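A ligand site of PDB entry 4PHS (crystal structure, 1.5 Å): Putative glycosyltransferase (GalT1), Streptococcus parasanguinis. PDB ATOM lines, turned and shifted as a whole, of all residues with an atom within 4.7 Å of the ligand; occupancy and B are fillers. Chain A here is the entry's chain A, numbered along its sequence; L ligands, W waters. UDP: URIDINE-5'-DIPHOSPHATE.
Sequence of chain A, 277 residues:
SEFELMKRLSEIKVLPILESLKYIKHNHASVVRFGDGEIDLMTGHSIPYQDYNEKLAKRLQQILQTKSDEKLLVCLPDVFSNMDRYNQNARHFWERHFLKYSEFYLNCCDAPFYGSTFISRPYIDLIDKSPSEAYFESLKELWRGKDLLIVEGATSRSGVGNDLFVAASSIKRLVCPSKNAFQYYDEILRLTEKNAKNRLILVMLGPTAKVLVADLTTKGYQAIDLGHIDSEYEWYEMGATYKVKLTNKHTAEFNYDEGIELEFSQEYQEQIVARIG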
ATOM      1  N   ARG A  33      17.939 -15.016  31.697  1.00  0.00           N
ATOM      2  CA  ARG A  33      17.186 -13.876  31.201  1.00  0.00           C
ATOM      3  C   ARG A  33      16.578 -14.120  29.817  1.00  0.00           C
ATOM      4  O   ARG A  33      17.230 -14.662  28.940  1.00  0.00           O
ATOM      5  CB  ARG A  33      18.078 -12.623  31.153  1.00  0.00           C
ATOM      6  CG  ARG A  33      18.803 -12.270  32.462  1.00  0.00           C
ATOM      7  CD  ARG A  33      19.825 -11.093  32.249  1.00  0.00           C
ATOM      8  NE  ARG A  33      20.741 -11.495  31.197  1.00  0.00           N
ATOM      9  CZ  ARG A  33      20.667 -11.149  29.915  1.00  0.00           C
ATOM     10  NH1 ARG A  33      21.501 -11.713  29.072  1.00  0.00           N
ATOM     11  NH2 ARG A  33      19.773 -10.264  29.480  1.00  0.00           N
ATOM     12  N   TYR A  49      22.924 -13.539  15.963  1.00  0.00           N
ATOM     13  CA  TYR A  49      23.975 -14.475  16.394  1.00  0.00           C
ATOM     14  C   TYR A  49      23.523 -15.894  16.781  1.00  0.00           C
ATOM     15  O   TYR A  49      24.239 -16.614  17.468  1.00  0.00           O
ATOM     16  CB  TYR A  49      24.916 -13.871  17.467  1.00  0.00           C
ATOM     17  CG  TYR A  49      24.296 -13.105  18.630  1.00  0.00           C
ATOM     18  CD1 TYR A  49      23.230 -13.623  19.357  1.00  0.00           C
ATOM     19  CD2 TYR A  49      24.840 -11.890  19.038  1.00  0.00           C
ATOM     20  CE1 TYR A  49      22.677 -12.921  20.422  1.00  0.00           C
ATOM     21  CE2 TYR A  49      24.308 -11.183  20.103  1.00  0.00           C
ATOM     22  CZ  TYR A  49      23.238 -11.700  20.793  1.00  0.00           C
ATOM     23  OH  TYR A  49      22.718 -10.980  21.845  1.00  0.00           O
ATOM     24  N   GLN A  50      22.339 -16.293  16.328  1.00  0.00           N
ATOM     25  CA  GLN A  50      21.905 -17.664  16.554  1.00  0.00           C
ATOM     26  C   GLN A  50      20.796 -18.018  15.571  1.00  0.00           C
ATOM     27  O   GLN A  50      19.707 -17.451  15.605  1.00  0.00           O
ATOM     28  CB  GLN A  50      21.438 -17.884  17.996  1.00  0.00           C
ATOM     29  CG  GLN A  50      20.935 -19.288  18.278  1.00  0.00           C
ATOM     30  CD  GLN A  50      21.993 -20.335  18.013  1.00  0.00           C
ATOM     31  OE1 GLN A  50      23.051 -20.331  18.649  1.00  0.00           O
ATOM     32  NE2 GLN A  50      21.733 -21.229  17.060  1.00  0.00           N
ATOM     33  N   THR A 117      15.348  -8.814  32.938  1.00  0.00           N
ATOM     34  CA  THR A 117      16.296  -9.100  31.877  1.00  0.00           C
ATOM     35  C   THR A 117      17.293  -7.951  31.746  1.00  0.00           C
ATOM     36  O   THR A 117      18.404  -8.133  31.256  1.00  0.00           O
ATOM     37  CB  THR A 117      15.538  -9.363  30.575  1.00  0.00           C
ATOM     38  OG1 THR A 117      14.851 -10.621  30.707  1.00  0.00           O
ATOM     39  CG2 THR A 117      16.449  -9.402  29.359  1.00  0.00           C
ATOM     40  N   SER A 120      21.483  -6.908  32.790  1.00  0.00           N
ATOM     41  CA  SER A 120      22.643  -6.781  31.902  1.00  0.00           C
ATOM     42  C   SER A 120      22.605  -5.496  31.106  1.00  0.00           C
ATOM     43  O   SER A 120      23.580  -5.165  30.415  1.00  0.00           O
ATOM     44  CB  SER A 120      22.674  -7.926  30.896  1.00  0.00           C
ATOM     45  OG  SER A 120      21.498  -7.892  30.106  1.00  0.00           O
ATOM     46  N   ARG A 121      21.479  -4.781  31.184  1.00  0.00           N
ATOM     47  CA  ARG A 121      21.261  -3.576  30.373  1.00  0.00           C
ATOM     48  C   ARG A 121      20.876  -2.397  31.258  1.00  0.00           C
ATOM     49  O   ARG A 121      19.730  -1.927  31.234  1.00  0.00           O
ATOM     50  CB  ARG A 121      20.163  -3.841  29.325  1.00  0.00           C
ATOM     51  CG  ARG A 121      20.251  -5.167  28.580  1.00  0.00           C
ATOM     52  CD  ARG A 121      21.490  -5.302  27.727  1.00  0.00           C
ATOM     53  NE  ARG A 121      21.645  -4.125  26.879  1.00  0.00           N
ATOM     54  CZ  ARG A 121      21.682  -4.139  25.552  1.00  0.00           C
ATOM     55  NH1 ARG A 121      21.597  -5.284  24.885  1.00  0.00           N
ATOM     56  NH2 ARG A 121      21.813  -2.992  24.907  1.00  0.00           N
ATOM     57  N   GLU A 152      31.826 -17.244  27.440  1.00  0.00           N
ATOM     58  CA  GLU A 152      31.428 -16.153  26.540  1.00  0.00           C
ATOM     59  C   GLU A 152      31.973 -16.432  25.144  1.00  0.00           C
ATOM     60  O   GLU A 152      32.715 -17.398  24.947  1.00  0.00           O
ATOM     61  CB  GLU A 152      31.984 -14.812  27.054  1.00  0.00           C
ATOM     62  CG  GLU A 152      33.508 -14.777  27.010  1.00  0.00           C
ATOM     63  CD  GLU A 152      34.119 -13.453  27.461  1.00  0.00           C
ATOM     64  OE1 GLU A 152      33.379 -12.498  27.827  1.00  0.00           O
ATOM     65  OE2 GLU A 152      35.363 -13.371  27.439  1.00  0.00           O
ATOM     66  N   GLY A 153      31.620 -15.575  24.198  1.00  0.00           N
ATOM     67  CA  GLY A 153      32.070 -15.767  22.826  1.00  0.00           C
ATOM     68  C   GLY A 153      33.409 -15.128  22.547  1.00  0.00           C
ATOM     69  O   GLY A 153      33.923 -14.366  23.363  1.00  0.00           O
ATOM     70  N   THR A 155      34.289 -12.778  20.537  1.00  0.00           N
ATOM     71  CA  THR A 155      34.296 -11.327  20.432  1.00  0.00           C
ATOM     72  C   THR A 155      33.770 -10.628  21.679  1.00  0.00           C
ATOM     73  O   THR A 155      33.927  -9.405  21.823  1.00  0.00           O
ATOM     74  CB  THR A 155      33.518 -10.829  19.209  1.00  0.00           C
ATOM     75  OG1 THR A 155      32.149 -11.228  19.311  1.00  0.00           O
ATOM     76  CG2 THR A 155      34.122 -11.412  17.948  1.00  0.00           C
ATOM     77  N   SER A 156      33.198 -11.404  22.611  1.00  0.00           N
ATOM     78  CA  SER A 156      32.570 -10.827  23.805  1.00  0.00           C
ATOM     79  C   SER A 156      33.556 -10.028  24.647  1.00  0.00           C
ATOM     80  O   SER A 156      33.284  -8.880  24.998  1.00  0.00           O
ATOM     81  CB  SER A 156      31.950 -11.935  24.657  1.00  0.00           C
ATOM     82  OG  SER A 156      30.887 -12.579  23.975  1.00  0.00           O
ATOM     83  N   PRO A 177      31.976 -19.972  20.275  1.00  0.00           N
ATOM     84  CA  PRO A 177      31.740 -19.178  19.058  1.00  0.00           C
ATOM     85  C   PRO A 177      30.916 -17.909  19.301  1.00  0.00           C
ATOM     86  O   PRO A 177      30.029 -17.915  20.160  1.00  0.00           O
ATOM     87  CB  PRO A 177      30.973 -20.146  18.151  1.00  0.00           C
ATOM     88  CG  PRO A 177      31.381 -21.490  18.596  1.00  0.00           C
ATOM     89  CD  PRO A 177      31.528 -21.374  20.097  1.00  0.00           C
ATOM     90  N   SER A 178      31.219 -16.848  18.551  1.00  0.00           N
ATOM     91  CA  SER A 178      30.587 -15.543  18.720  1.00  0.00           C
ATOM     92  C   SER A 178      29.164 -15.561  18.144  1.00  0.00           C
ATOM     93  O   SER A 178      28.343 -14.716  18.463  1.00  0.00           O
ATOM     94  CB  SER A 178      31.402 -14.451  18.032  1.00  0.00           C
ATOM     95  OG  SER A 178      31.635 -14.791  16.674  1.00  0.00           O
ATOM     96  N   LYS A 179      28.901 -16.538  17.282  1.00  0.00           N
ATOM     97  CA  LYS A 179      27.568 -16.725  16.706  1.00  0.00           C
ATOM     98  C   LYS A 179      27.298 -18.216  16.649  1.00  0.00           C
ATOM     99  O   LYS A 179      28.235 -19.019  16.462  1.00  0.00           O
ATOM    100  CB  LYS A 179      27.503 -16.161  15.287  1.00  0.00           C
ATOM    101  CG  LYS A 179      27.616 -14.661  15.149  1.00  0.00           C
ATOM    102  CD  LYS A 179      27.624 -14.308  13.662  1.00  0.00           C
ATOM    103  CE  LYS A 179      27.482 -12.820  13.412  1.00  0.00           C
ATOM    104  NZ  LYS A 179      27.290 -12.563  11.958  1.00  0.00           N
ATOM    105  N   ASN A 180      26.026 -18.597  16.773  1.00  0.00           N
ATOM    106  CA  ASN A 180      25.641 -20.000  16.632  1.00  0.00           C
ATOM    107  C   ASN A 180      26.394 -20.939  17.572  1.00  0.00           C
ATOM    108  O   ASN A 180      26.774 -22.052  17.206  1.00  0.00           O
ATOM    109  CB  ASN A 180      25.786 -20.435  15.171  1.00  0.00           C
ATOM    110  CG  ASN A 180      24.695 -19.845  14.307  1.00  0.00           C
ATOM    111  OD1 ASN A 180      23.533 -19.844  14.700  1.00  0.00           O
ATOM    112  ND2 ASN A 180      25.065 -19.320  13.141  1.00  0.00           N
ATOM    113  N   ALA A 181      26.624 -20.449  18.785  1.00  0.00           N
ATOM    114  CA  ALA A 181      27.267 -21.262  19.795  1.00  0.00           C
ATOM    115  C   ALA A 181      26.477 -22.528  20.077  1.00  0.00           C
ATOM    116  O   ALA A 181      27.042 -23.507  20.556  1.00  0.00           O
ATOM    117  CB  ALA A 181      27.476 -20.456  21.072  1.00  0.00           C
ATOM    118  N   MET A 204      27.885 -15.171  29.042  1.00  0.00           N
ATOM    119  CA  MET A 204      27.526 -14.149  28.059  1.00  0.00           C
ATOM    120  C   MET A 204      27.513 -14.803  26.691  1.00  0.00           C
ATOM    121  O   MET A 204      28.538 -14.852  26.014  1.00  0.00           O
ATOM    122  CB  MET A 204      28.531 -12.991  28.105  1.00  0.00           C
ATOM    123  CG  MET A 204      28.594 -12.245  29.451  1.00  0.00           C
ATOM    124  SD  MET A 204      29.537 -13.258  30.852  1.00  0.00           S
ATOM    125  CE  MET A 204      30.274 -11.760  31.873  1.00  0.00           C
ATOM    126  N   LEU A 205      26.372 -15.356  26.322  1.00  0.00           N
ATOM    127  CA  LEU A 205      26.361 -16.279  25.176  1.00  0.00           C
ATOM    128  C   LEU A 205      24.985 -16.378  24.519  1.00  0.00           C
ATOM    129  O   LEU A 205      24.577 -17.445  24.075  1.00  0.00           O
ATOM    130  CB  LEU A 205      26.854 -17.658  25.607  1.00  0.00           C
ATOM    131  CG  LEU A 205      27.559 -18.496  24.532  1.00  0.00           C
ATOM    132  CD1 LEU A 205      28.913 -17.903  24.201  1.00  0.00           C
ATOM    133  CD2 LEU A 205      27.717 -19.959  24.975  1.00  0.00           C
ATOM    134  N   GLY A 206      24.247 -15.266  24.472  1.00  0.00           N
ATOM    135  CA  GLY A 206      23.001 -15.227  23.722  1.00  0.00           C
ATOM    136  C   GLY A 206      22.031 -16.308  24.160  1.00  0.00           C
ATOM    137  O   GLY A 206      21.974 -16.643  25.337  1.00  0.00           O
ATOM    138  N   PRO A 207      21.266 -16.877  23.214  1.00  0.00           N
ATOM    139  CA  PRO A 207      20.274 -17.866  23.625  1.00  0.00           C
ATOM    140  C   PRO A 207      20.880 -19.128  24.222  1.00  0.00           C
ATOM    141  O   PRO A 207      20.238 -19.774  25.062  1.00  0.00           O
ATOM    142  CB  PRO A 207      19.557 -18.214  22.313  1.00  0.00           C
ATOM    143  CG  PRO A 207      19.770 -17.031  21.440  1.00  0.00           C
ATOM    144  CD  PRO A 207      21.136 -16.506  21.796  1.00  0.00           C
ATOM    145  N   LYS A 210      21.124 -19.290  28.076  1.00  0.00           N
ATOM    146  CA  LYS A 210      19.943 -19.614  28.863  1.00  0.00           C
ATOM    147  C   LYS A 210      19.861 -21.128  29.149  1.00  0.00           C
ATOM    148  O   LYS A 210      19.549 -21.527  30.266  1.00  0.00           O
ATOM    149  CB  LYS A 210      18.641 -19.174  28.171  1.00  0.00           C
ATOM    150  CG  LYS A 210      18.745 -17.981  27.219  1.00  0.00           C
ATOM    151  CD  LYS A 210      19.183 -16.742  27.934  1.00  0.00           C
ATOM    152  CE  LYS A 210      19.303 -15.601  26.954  1.00  0.00           C
ATOM    153  NZ  LYS A 210      20.113 -14.518  27.584  1.00  0.00           N
ATOM    154  N   ASP A 225      23.488 -15.432  33.965  1.00  0.00           N
ATOM    155  CA  ASP A 225      23.399 -14.976  32.582  1.00  0.00           C
ATOM    156  C   ASP A 225      23.537 -13.439  32.555  1.00  0.00           C
ATOM    157  O   ASP A 225      22.613 -12.702  32.952  1.00  0.00           O
ATOM    158  CB  ASP A 225      22.046 -15.427  32.029  1.00  0.00           C
ATOM    159  CG  ASP A 225      21.690 -14.814  30.696  1.00  0.00           C
ATOM    160  OD1 ASP A 225      22.551 -14.261  30.013  1.00  0.00           O
ATOM    161  OD2 ASP A 225      20.500 -14.946  30.309  1.00  0.00           O
ATOM    162  N   LEU A 226      24.690 -12.955  32.087  1.00  0.00           N
ATOM    163  CA  LEU A 226      24.985 -11.525  32.131  1.00  0.00           C
ATOM    164  C   LEU A 226      25.056 -10.870  30.750  1.00  0.00           C
ATOM    165  O   LEU A 226      25.268  -9.660  30.656  1.00  0.00           O
ATOM    166  CB  LEU A 226      26.278 -11.256  32.892  1.00  0.00           C
ATOM    167  CG  LEU A 226      26.159 -11.448  34.402  1.00  0.00           C
ATOM    168  CD1 LEU A 226      27.456 -11.032  35.069  1.00  0.00           C
ATOM    169  CD2 LEU A 226      25.003 -10.626  34.904  1.00  0.00           C
ATOM    170  N   GLY A 227      24.886 -11.652  29.691  1.00  0.00           N
ATOM    171  CA  GLY A 227      24.668 -11.090  28.366  1.00  0.00           C
ATOM    172  C   GLY A 227      25.585  -9.955  27.957  1.00  0.00           C
ATOM    173  O   GLY A 227      26.819 -10.110  27.927  1.00  0.00           O
ATOM    174  N   HIS A 228      24.975  -8.815  27.606  1.00  0.00           N
ATOM    175  CA  HIS A 228      25.721  -7.658  27.100  1.00  0.00           C
ATOM    176  C   HIS A 228      26.205  -6.670  28.165  1.00  0.00           C
ATOM    177  O   HIS A 228      26.421  -5.492  27.860  1.00  0.00           O
ATOM    178  CB  HIS A 228      24.837  -6.918  26.082  1.00  0.00           C
ATOM    179  CG  HIS A 228      24.880  -7.510  24.697  1.00  0.00           C
ATOM    180  ND1 HIS A 228      23.736  -7.895  24.034  1.00  0.00           N
ATOM    181  CD2 HIS A 228      25.908  -7.731  23.862  1.00  0.00           C
ATOM    182  CE1 HIS A 228      24.074  -8.375  22.844  1.00  0.00           C
ATOM    183  NE2 HIS A 228      25.383  -8.278  22.704  1.00  0.00           N
ATOM    184  N   HIS A 250      33.132  -7.044  20.496  1.00  0.00           N
ATOM    185  CA  HIS A 250      31.710  -7.037  20.193  1.00  0.00           C
ATOM    186  C   HIS A 250      31.000  -5.844  20.827  1.00  0.00           C
ATOM    187  O   HIS A 250      31.359  -5.392  21.925  1.00  0.00           O
ATOM    188  CB  HIS A 250      31.107  -8.339  20.715  1.00  0.00           C
ATOM    189  CG  HIS A 250      29.617  -8.407  20.593  1.00  0.00           C
ATOM    190  ND1 HIS A 250      28.974  -8.664  19.403  1.00  0.00           N
ATOM    191  CD2 HIS A 250      28.635  -8.270  21.522  1.00  0.00           C
ATOM    192  CE1 HIS A 250      27.672  -8.669  19.592  1.00  0.00           C
ATOM    193  NE2 HIS A 250      27.441  -8.436  20.873  1.00  0.00           N
ATOM    194  N   GLU A 253      23.967  -4.973  19.910  1.00  0.00           N
ATOM    195  CA  GLU A 253      23.106  -4.535  18.793  1.00  0.00           C
ATOM    196  C   GLU A 253      23.868  -4.149  17.524  1.00  0.00           C
ATOM    197  O   GLU A 253      23.276  -3.704  16.547  1.00  0.00           O
ATOM    198  CB  GLU A 253      22.112  -3.441  19.218  1.00  0.00           C
ATOM    199  CG  GLU A 253      20.969  -3.979  20.084  1.00  0.00           C
ATOM    200  CD  GLU A 253      21.382  -4.175  21.539  1.00  0.00           C
ATOM    201  OE1 GLU A 253      21.653  -3.161  22.200  1.00  0.00           O
ATOM    202  OE2 GLU A 253      21.428  -5.339  22.007  1.00  0.00           O
HETATM  203  N1  UDP L   1      27.074 -14.451  22.067  1.00  0.00           N
HETATM  204  C2  UDP L   1      28.075 -15.320  21.715  1.00  0.00           C
HETATM  205  N3  UDP L   1      27.787 -16.415  20.937  1.00  0.00           N
HETATM  206  C4  UDP L   1      26.495 -16.644  20.498  1.00  0.00           C
HETATM  207  C5  UDP L   1      25.479 -15.773  20.875  1.00  0.00           C
HETATM  208  C6  UDP L   1      25.813 -14.599  21.544  1.00  0.00           C
HETATM  209  O2  UDP L   1      29.228 -15.119  22.101  1.00  0.00           O
HETATM  210  O4  UDP L   1      26.228 -17.628  19.797  1.00  0.00           O
HETATM  211  C1' UDP L   1      27.395 -13.337  22.982  1.00  0.00           C
HETATM  212  C2' UDP L   1      27.541 -11.955  22.383  1.00  0.00           C
HETATM  213  O2' UDP L   1      28.809 -11.773  21.777  1.00  0.00           O
HETATM  214  C3' UDP L   1      27.380 -11.102  23.638  1.00  0.00           C
HETATM  215  C4' UDP L   1      26.390 -11.899  24.488  1.00  0.00           C
HETATM  216  O4' UDP L   1      26.332 -13.206  23.911  1.00  0.00           O
HETATM  217  O3' UDP L   1      28.608 -11.000  24.348  1.00  0.00           O
HETATM  218  C5' UDP L   1      24.987 -11.293  24.509  1.00  0.00           C
HETATM  219  O5' UDP L   1      24.124 -12.174  25.205  1.00  0.00           O
HETATM  220  PA  UDP L   1      22.559 -11.862  25.333  1.00  0.00           P
HETATM  221  O1A UDP L   1      22.021 -12.757  26.401  1.00  0.00           O
HETATM  222  O2A UDP L   1      21.864 -11.899  24.036  1.00  0.00           O
HETATM  223  O3A UDP L   1      22.622 -10.327  25.862  1.00  0.00           O
HETATM  224  PB  UDP L   1      21.497  -9.302  26.408  1.00  0.00           P
HETATM  225  O1B UDP L   1      22.133  -8.696  27.589  1.00  0.00           O
HETATM  226  O2B UDP L   1      20.210  -9.993  26.688  1.00  0.00           O
HETATM  227  O3B UDP L   1      21.342  -8.256  25.336  1.00  0.00           O
HETATM  228  O   HOH W   1      28.426 -12.236  19.057  1.00  0.00           O
HETATM  229  O   HOH W   2      19.990 -13.285  22.693  1.00  0.00           O
HETATM  230  O   HOH W   3      17.934  -9.114  25.436  1.00  0.00           O
HETATM  231  O   HOH W   4      23.734 -18.768  20.754  1.00  0.00           O
HETATM  232  O   HOH W   5      31.344 -13.157  20.984  1.00  0.00           O
HETATM  233  O   HOH W   6      20.401  -9.158  23.068  1.00  0.00           O
HETATM  234  O   HOH W   7      28.924  -8.641  25.481  1.00  0.00           O
HETATM  235  O   HOH W   8      18.561 -12.265  26.800  1.00  0.00           O
HETATM  236  O   HOH W   9      24.063 -14.250  27.759  1.00  0.00           O
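An oxygen (O4') of the ligand sits close to the backbone carbonyl oxygen of Met 204 (3.5 Å).
C of Lys 179 touches O4 of the ligand, at 3.4 Å.
Asp 225 touches the ligand.
Gly 227 touches the ligand.
His 250 touches the ligand (CD2 to O2', 3.5 Å).
19 residues have an atom within 4 Å of the ligand: Arg 33, Tyr 49, Ser 120, Arg 121, Gly 153, Ser 156, Pro 177, Ser 178, Lys 179, Asn 180, Ala 181, Met 204, Leu 205, Gly 206, Lys 210, Asp 225, Gly 227, His 228 and His 250.
The side-chain hydroxyl (OG) of Ser 120 sits at hydrogen-bond distance from the backbone carbonyl oxygen (O) of Thr 117, 3.3 Å away.
NH2 of Arg 33 sits at hydrogen-bond distance from O of Thr 117 (3.1 Å).
NH1 of Arg 33 lies within salt-bridge range of OD1 of Asp 225.
The side-chain amino group of Lys 210 is in salt-bridge range of the side-chain carboxylate of Asp 225.
The side-chain amide oxygen (OD1) of Asn 180 lies within hydrogen-bond range of the side-chain amide nitrogen (NE2) of Gln 50 (3.3 Å).
A ring nitrogen (NE2) of His 228 lies within hydrogen-bond range of a ring nitrogen (NE2) of His 250 (2.8 Å).
A ring nitrogen (ND1) of His 228 lies within hydrogen-bond range of the guanidinium group (NH1) of Arg 121, 3.5 Å away.
The side-chain hydroxyl (OG) of Ser 156 sits at hydrogen-bond distance from the backbone NH (N) of Gly 153, 3.1 Å away.
N of Ala 181 is in hydrogen-bond range of O4 of the ligand (3.0 Å).
OG of Ser 120 sits at hydrogen-bond distance from O1B of the ligand, at 2.7 Å.
N of Gly 153 lies close to O2 of the ligand (3.2 Å).
O1B of the ligand lies within hydrogen-bond range of N of His 228 (2.8 Å).
OG of Ser 156 lies within hydrogen-bond range of O3' of the ligand (2.8 Å).
The guanidinium group (NH1) of Arg 121 lies within salt-bridge range of an oxygen (O3B) of the ligand (3.0 Å).
ND1 of His 228 lies within hydrogen-bond range of O3B of the ligand.
The backbone carbonyl oxygen of Ser 178 is in hydrogen-bond range of a nitrogen (N3) of the ligand (3.1 Å).
N of Asn 180 sits at hydrogen-bond distance from O4 of the ligand, at 3.2 Å.
The backbone NH (N) of Leu 205 sits at hydrogen-bond distance from an oxygen (O4') of the ligand.
The backbone carbonyl oxygen of Pro 177 is in hydrogen-bond range of a nitrogen (N3) of the ligand.
The side-chain amino group (NZ) of Lys 210 is in salt-bridge range of an oxygen (O1A) of the ligand (2.9 Å).
The backbone NH (N) of Gly 206 sits at hydrogen-bond distance from an oxygen (O4') of the ligand.
An oxygen (O2A) of the ligand is in hydrogen-bond range of the side-chain hydroxyl of Tyr 49 (2.5 Å).
NH2 of Arg 33 lies within salt-bridge range of O2B of the ligand, at 2.8 Å.
Water W6 bridges an oxygen (O3B) of the ligand (2.6 Å) and the side-chain hydroxyl of Tyr 49 (3.2 Å).
Water W1 lies within hydrogen-bond range of the backbone carbonyl oxygen (O) of Ser 178 and an oxygen (O2') of the ligand.
Water W8 lies within hydrogen-bond range of O2B of the ligand (2.8 Å), NZ of Lys 210 (2.8 Å) and O of Arg 33 (3.5 Å).
Water W4 bridges OE1 of Gln 50 (2.7 Å) and O4 of the ligand (2.9 Å).
Water W5 lies within hydrogen-bond range of the side-chain hydroxyl (OG1) of Thr 155 (2.7 Å), an oxygen (O2') of the ligand (3.0 Å) and the backbone NH (N) of Ser 156 (3.0 Å).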
